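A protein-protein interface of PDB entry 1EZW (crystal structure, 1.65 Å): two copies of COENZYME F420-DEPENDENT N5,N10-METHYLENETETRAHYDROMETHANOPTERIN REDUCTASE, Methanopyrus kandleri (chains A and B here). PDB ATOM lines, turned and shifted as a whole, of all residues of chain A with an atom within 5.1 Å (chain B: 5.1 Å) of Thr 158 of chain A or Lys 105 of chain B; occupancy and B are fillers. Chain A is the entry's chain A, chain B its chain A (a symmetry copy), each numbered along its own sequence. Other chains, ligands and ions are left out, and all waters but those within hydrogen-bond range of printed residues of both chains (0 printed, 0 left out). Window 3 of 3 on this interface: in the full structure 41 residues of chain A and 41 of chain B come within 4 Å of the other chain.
Tyr 40 of chain B touches Leu 74 of chain A.
Met 106 of chain B touches Leu 74 of chain A.
Thr 156 of chain A touches Lys 105 of chain B (C to O, 3.96 Å).
Thr 156 of chain A touches Met 106 of chain B.
Asp 104 of chain B touches Gly 157 of chain A (O to CA, 3.5 Å).
N of Gly 157 of chain A touches C of Met 106 of chain B, 3.9 Å away.
N of Gly 107 of chain B touches N of Gly 157 of chain A, 3.7 Å away.
Thr 158 of chain A touches Lys 105 of chain B (O to CG, 3.5 Å).
Lys 105 of chain B touches Ala 159 of chain A (O to CB, 3.5 Å).
Asn 41 of chain B touches Asp 160 of chain A (CB to O, 3.2 Å).
The side-chain hydroxyl of Thr 158 of chain A is in hydrogen-bond range of the side-chain carboxylate of Glu 148 of chain A (2.8 Å).
OD2 of Asp 104 of chain B lies within salt-bridge range of NZ of Lys 100 of chain B (2.9 Å).
N of Val 147 of chain A sits at hydrogen-bond distance from O of Ala 159 of chain A (2.8 Å).
No position is printed for both chains.
The side-chain carboxylate of Asp 160 of chain A lies within salt-bridge range of the side-chain amino group of Lys 105 of chain B (2.9 Å).
O of Asp 160 of chain A is in hydrogen-bond range of OH of Tyr 40 of chain B, at 2.6 Å.
O of Lys 105 of chain B lies within hydrogen-bond range of N of Gly 157 of chain A (2.8 Å).
Thr 158 of chain A touches just one residue of chain B: Lys 105.
Of chain A, only Thr 156 (3.96 Å), Gly 157 (2.8 Å), Thr 158 (3.5 Å), Ala 159 (3.5 Å) and Asp 160 (2.9 Å) come within 4 Å of Lys 105 of chain B.
Of the printed residues of chain B, Leu 74 of chain A touches Tyr 40 and Met 106.
Printed residues of chain B within 4 Å of Thr 156 of chain A: Lys 105 (3.96 Å) and Met 106 (3.3 Å).
Of the printed residues of chain B, Gly 157 of chain A touches Asp 104 (3.5 Å), Lys 105 (2.8 Å), Met 106 (3.9 Å) and Gly 107 (3.7 Å).
Of the printed residues of chain A, Asp 104 of chain B touches Gly 157.
Of the printed residues of chain A, Tyr 40 of chain B touches Leu 74 (3.7 Å), Ala 159 (3.2 Å) and Asp 160 (2.6 Å).
Pro 146 of chain A touches none of the printed residues of chain B.
Of the 9 printed residues of chain A, 6 touch a printed residue of chain B.
Of the 10 printed residues of chain B, 6 touch a printed residue of chain A.
Hydrophobic or aromatic side chains of chain B within 4 Å of the printed part of chain A: Tyr 40.
Among the printed residues, 14 pairs touch across the chains.
Among the printed residues, Asp or Glu carboxylates within 4 Å of a Lys or Arg side-chain nitrogen of the other chain: Asp 160 of chain A with Lys 105 of chain B (2.9 Å).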
ATOM      1  N   LEU A  74      -1.287 -25.139 -33.015  1.00  0.00           N
ATOM      2  CA  LEU A  74      -0.848 -24.989 -31.635  1.00  0.00           C
ATOM      3  C   LEU A  74      -1.396 -26.175 -30.828  1.00  0.00           C
ATOM      4  O   LEU A  74      -0.788 -26.567 -29.843  1.00  0.00           O
ATOM      5  CB  LEU A  74      -1.363 -23.673 -31.015  1.00  0.00           C
ATOM      6  CG  LEU A  74      -0.584 -22.441 -31.513  1.00  0.00           C
ATOM      7  CD1 LEU A  74      -1.317 -21.147 -31.030  1.00  0.00           C
ATOM      8  CD2 LEU A  74       0.866 -22.471 -30.953  1.00  0.00           C
ATOM      9  N   PRO A 146       7.424 -17.596 -26.545  1.00  0.00           N
ATOM     10  CA  PRO A 146       6.061 -17.551 -27.070  1.00  0.00           C
ATOM     11  C   PRO A 146       6.056 -17.771 -28.583  1.00  0.00           C
ATOM     12  O   PRO A 146       6.987 -17.369 -29.301  1.00  0.00           O
ATOM     13  CB  PRO A 146       5.596 -16.142 -26.699  1.00  0.00           C
ATOM     14  CG  PRO A 146       6.918 -15.373 -26.825  1.00  0.00           C
ATOM     15  CD  PRO A 146       7.793 -16.278 -25.996  1.00  0.00           C
ATOM     16  N   VAL A 147       5.023 -18.430 -29.075  1.00  0.00           N
ATOM     17  CA  VAL A 147       4.946 -18.619 -30.500  1.00  0.00           C
ATOM     18  C   VAL A 147       4.388 -17.320 -31.100  1.00  0.00           C
ATOM     19  O   VAL A 147       3.399 -16.805 -30.630  1.00  0.00           O
ATOM     20  CB  VAL A 147       3.990 -19.742 -30.859  1.00  0.00           C
ATOM     21  CG1 VAL A 147       3.931 -19.870 -32.365  1.00  0.00           C
ATOM     22  CG2 VAL A 147       4.428 -21.041 -30.170  1.00  0.00           C
ATOM     23  N   GLU A 148       5.060 -16.782 -32.112  1.00  0.00           N
ATOM     24  CA  GLU A 148       4.597 -15.576 -32.787  1.00  0.00           C
ATOM     25  C   GLU A 148       4.883 -15.862 -34.225  1.00  0.00           C
ATOM     26  O   GLU A 148       6.044 -15.930 -34.640  1.00  0.00           O
ATOM     27  CB  GLU A 148       5.362 -14.345 -32.303  1.00  0.00           C
ATOM     28  CG  GLU A 148       4.973 -13.942 -30.881  1.00  0.00           C
ATOM     29  CD  GLU A 148       5.688 -12.676 -30.407  1.00  0.00           C
ATOM     30  OE1 GLU A 148       5.016 -11.777 -29.852  1.00  0.00           O
ATOM     31  OE2 GLU A 148       6.918 -12.594 -30.580  1.00  0.00           O
ATOM     32  N   THR A 156      -0.811 -16.375 -35.686  1.00  0.00           N
ATOM     33  CA  THR A 156      -1.078 -16.452 -34.251  1.00  0.00           C
ATOM     34  C   THR A 156      -0.992 -15.070 -33.627  1.00  0.00           C
ATOM     35  O   THR A 156      -0.601 -14.084 -34.293  1.00  0.00           O
ATOM     36  CB  THR A 156      -0.013 -17.292 -33.531  1.00  0.00           C
ATOM     37  OG1 THR A 156       1.241 -16.598 -33.520  1.00  0.00           O
ATOM     38  CG2 THR A 156       0.188 -18.638 -34.232  1.00  0.00           C
ATOM     39  N   GLY A 157      -1.402 -14.992 -32.366  1.00  0.00           N
ATOM     40  CA  GLY A 157      -1.219 -13.788 -31.581  1.00  0.00           C
ATOM     41  C   GLY A 157       0.092 -14.087 -30.853  1.00  0.00           C
ATOM     42  O   GLY A 157       0.948 -14.795 -31.379  1.00  0.00           O
ATOM     43  N   THR A 158       0.303 -13.549 -29.655  1.00  0.00           N
ATOM     44  CA  THR A 158       1.527 -13.860 -28.914  1.00  0.00           C
ATOM     45  C   THR A 158       1.130 -15.013 -28.019  1.00  0.00           C
ATOM     46  O   THR A 158       0.566 -14.828 -26.951  1.00  0.00           O
ATOM     47  CB  THR A 158       1.979 -12.652 -28.100  1.00  0.00           C
ATOM     48  OG1 THR A 158       2.337 -11.626 -29.045  1.00  0.00           O
ATOM     49  CG2 THR A 158       3.163 -12.990 -27.245  1.00  0.00           C
ATOM     50  N   ALA A 159       1.466 -16.218 -28.467  1.00  0.00           N
ATOM     51  CA  ALA A 159       1.016 -17.415 -27.764  1.00  0.00           C
ATOM     52  C   ALA A 159       2.036 -18.005 -26.804  1.00  0.00           C
ATOM     53  O   ALA A 159       2.928 -18.728 -27.227  1.00  0.00           O
ATOM     54  CB  ALA A 159       0.612 -18.452 -28.801  1.00  0.00           C
ATOM     55  N   ASP A 160       1.912 -17.680 -25.517  1.00  0.00           N
ATOM     56  CA  ASP A 160       2.843 -18.200 -24.554  1.00  0.00           C
ATOM     57  C   ASP A 160       2.603 -19.701 -24.425  1.00  0.00           C
ATOM     58  O   ASP A 160       1.542 -20.225 -24.823  1.00  0.00           O
ATOM     59  CB  ASP A 160       2.688 -17.475 -23.217  1.00  0.00           C
ATOM     60  CG  ASP A 160       1.357 -17.712 -22.573  1.00  0.00           C
ATOM     61  OD1 ASP A 160       0.308 -17.625 -23.245  1.00  0.00           O
ATOM     62  OD2 ASP A 160       1.351 -17.965 -21.354  1.00  0.00           O
ATOM     63  N   TYR B  40      -4.323 -24.648 -25.543  1.00  0.00           N
ATOM     64  CA  TYR B  40      -3.139 -25.079 -26.285  1.00  0.00           C
ATOM     65  C   TYR B  40      -1.838 -24.853 -25.519  1.00  0.00           C
ATOM     66  O   TYR B  40      -0.844 -25.561 -25.744  1.00  0.00           O
ATOM     67  CB  TYR B  40      -3.062 -24.332 -27.645  1.00  0.00           C
ATOM     68  CG  TYR B  40      -2.465 -22.954 -27.466  1.00  0.00           C
ATOM     69  CD1 TYR B  40      -1.073 -22.781 -27.475  1.00  0.00           C
ATOM     70  CD2 TYR B  40      -3.270 -21.881 -27.021  1.00  0.00           C
ATOM     71  CE1 TYR B  40      -0.478 -21.606 -27.017  1.00  0.00           C
ATOM     72  CE2 TYR B  40      -2.676 -20.685 -26.558  1.00  0.00           C
ATOM     73  CZ  TYR B  40      -1.299 -20.563 -26.543  1.00  0.00           C
ATOM     74  OH  TYR B  40      -0.710 -19.455 -25.958  1.00  0.00           O
ATOM     75  N   ASN B  41      -1.820 -23.869 -24.609  1.00  0.00           N
ATOM     76  CA  ASN B  41      -0.565 -23.578 -23.931  1.00  0.00           C
ATOM     77  C   ASN B  41      -0.181 -24.581 -22.861  1.00  0.00           C
ATOM     78  O   ASN B  41       0.946 -24.600 -22.398  1.00  0.00           O
ATOM     79  CB  ASN B  41      -0.582 -22.160 -23.316  1.00  0.00           C
ATOM     80  CG  ASN B  41      -1.793 -21.910 -22.446  1.00  0.00           C
ATOM     81  OD1 ASN B  41      -2.919 -22.064 -22.882  1.00  0.00           O
ATOM     82  ND2 ASN B  41      -1.559 -21.490 -21.221  1.00  0.00           N
ATOM     83  N   LYS B 100     -11.725 -15.844 -24.563  1.00  0.00           N
ATOM     84  CA  LYS B 100     -11.002 -14.727 -25.116  1.00  0.00           C
ATOM     85  C   LYS B 100      -9.481 -14.729 -24.953  1.00  0.00           C
ATOM     86  O   LYS B 100      -8.751 -14.564 -25.946  1.00  0.00           O
ATOM     87  CB  LYS B 100     -11.558 -13.401 -24.541  1.00  0.00           C
ATOM     88  CG  LYS B 100     -10.851 -12.192 -25.113  1.00  0.00           C
ATOM     89  CD  LYS B 100     -11.333 -10.876 -24.464  1.00  0.00           C
ATOM     90  CE  LYS B 100     -10.489  -9.694 -24.917  1.00  0.00           C
ATOM     91  NZ  LYS B 100     -10.361  -9.563 -26.411  1.00  0.00           N
ATOM     92  N   ALA B 101      -9.000 -14.927 -23.730  1.00  0.00           N
ATOM     93  CA  ALA B 101      -7.561 -14.855 -23.494  1.00  0.00           C
ATOM     94  C   ALA B 101      -6.825 -15.863 -24.353  1.00  0.00           C
ATOM     95  O   ALA B 101      -5.811 -15.539 -24.983  1.00  0.00           O
ATOM     96  CB  ALA B 101      -7.250 -15.077 -22.002  1.00  0.00           C
ATOM     97  N   THR B 102      -7.360 -17.077 -24.405  1.00  0.00           N
ATOM     98  CA  THR B 102      -6.695 -18.120 -25.194  1.00  0.00           C
ATOM     99  C   THR B 102      -6.858 -17.928 -26.698  1.00  0.00           C
ATOM    100  O   THR B 102      -5.878 -18.058 -27.443  1.00  0.00           O
ATOM    101  CB  THR B 102      -7.190 -19.529 -24.777  1.00  0.00           C
ATOM    102  OG1 THR B 102      -7.067 -19.658 -23.352  1.00  0.00           O
ATOM    103  CG2 THR B 102      -6.303 -20.622 -25.436  1.00  0.00           C
ATOM    104  N   PHE B 103      -8.068 -17.613 -27.160  1.00  0.00           N
ATOM    105  CA  PHE B 103      -8.262 -17.393 -28.593  1.00  0.00           C
ATOM    106  C   PHE B 103      -7.438 -16.212 -29.103  1.00  0.00           C
ATOM    107  O   PHE B 103      -6.844 -16.290 -30.181  1.00  0.00           O
ATOM    108  CB  PHE B 103      -9.753 -17.250 -28.915  1.00  0.00           C
ATOM    109  CG  PHE B 103     -10.450 -18.567 -29.130  1.00  0.00           C
ATOM    110  CD1 PHE B 103     -10.071 -19.719 -28.413  1.00  0.00           C
ATOM    111  CD2 PHE B 103     -11.506 -18.662 -30.026  1.00  0.00           C
ATOM    112  CE1 PHE B 103     -10.742 -20.930 -28.593  1.00  0.00           C
ATOM    113  CE2 PHE B 103     -12.180 -19.870 -30.218  1.00  0.00           C
ATOM    114  CZ  PHE B 103     -11.801 -21.008 -29.501  1.00  0.00           C
ATOM    115  N   ASP B 104      -7.325 -15.130 -28.318  1.00  0.00           N
ATOM    116  CA  ASP B 104      -6.483 -14.027 -28.795  1.00  0.00           C
ATOM    117  C   ASP B 104      -5.036 -14.505 -29.023  1.00  0.00           C
ATOM    118  O   ASP B 104      -4.393 -14.164 -30.043  1.00  0.00           O
ATOM    119  CB  ASP B 104      -6.486 -12.849 -27.796  1.00  0.00           C
ATOM    120  CG  ASP B 104      -7.808 -12.080 -27.793  1.00  0.00           C
ATOM    121  OD1 ASP B 104      -8.585 -12.209 -28.754  1.00  0.00           O
ATOM    122  OD2 ASP B 104      -8.055 -11.320 -26.823  1.00  0.00           O
ATOM    123  N   LYS B 105      -4.534 -15.312 -28.087  1.00  0.00           N
ATOM    124  CA  LYS B 105      -3.173 -15.814 -28.204  1.00  0.00           C
ATOM    125  C   LYS B 105      -3.054 -16.685 -29.450  1.00  0.00           C
ATOM    126  O   LYS B 105      -2.061 -16.611 -30.141  1.00  0.00           O
ATOM    127  CB  LYS B 105      -2.774 -16.654 -26.977  1.00  0.00           C
ATOM    128  CG  LYS B 105      -2.545 -15.849 -25.683  1.00  0.00           C
ATOM    129  CD  LYS B 105      -2.382 -16.842 -24.534  1.00  0.00           C
ATOM    130  CE  LYS B 105      -2.275 -16.186 -23.162  1.00  0.00           C
ATOM    131  NZ  LYS B 105      -2.349 -17.294 -22.138  1.00  0.00           N
ATOM    132  N   MET B 106      -4.065 -17.508 -29.721  1.00  0.00           N
ATOM    133  CA  MET B 106      -4.013 -18.404 -30.879  1.00  0.00           C
ATOM    134  C   MET B 106      -4.150 -17.685 -32.208  1.00  0.00           C
ATOM    135  O   MET B 106      -3.703 -18.207 -33.224  1.00  0.00           O
ATOM    136  CB  MET B 106      -5.115 -19.456 -30.793  1.00  0.00           C
ATOM    137  CG  MET B 106      -4.998 -20.343 -29.572  1.00  0.00           C
ATOM    138  SD  MET B 106      -6.229 -21.649 -29.544  1.00  0.00           S
ATOM    139  CE  MET B 106      -5.419 -22.852 -30.707  1.00  0.00           C
ATOM    140  N   GLY B 107      -4.800 -16.521 -32.190  1.00  0.00           N
ATOM    141  CA  GLY B 107      -5.016 -15.759 -33.413  1.00  0.00           C
ATOM    142  C   GLY B 107      -6.442 -15.929 -33.914  1.00  0.00           C
ATOM    143  O   GLY B 107      -6.779 -15.509 -35.011  1.00  0.00           O
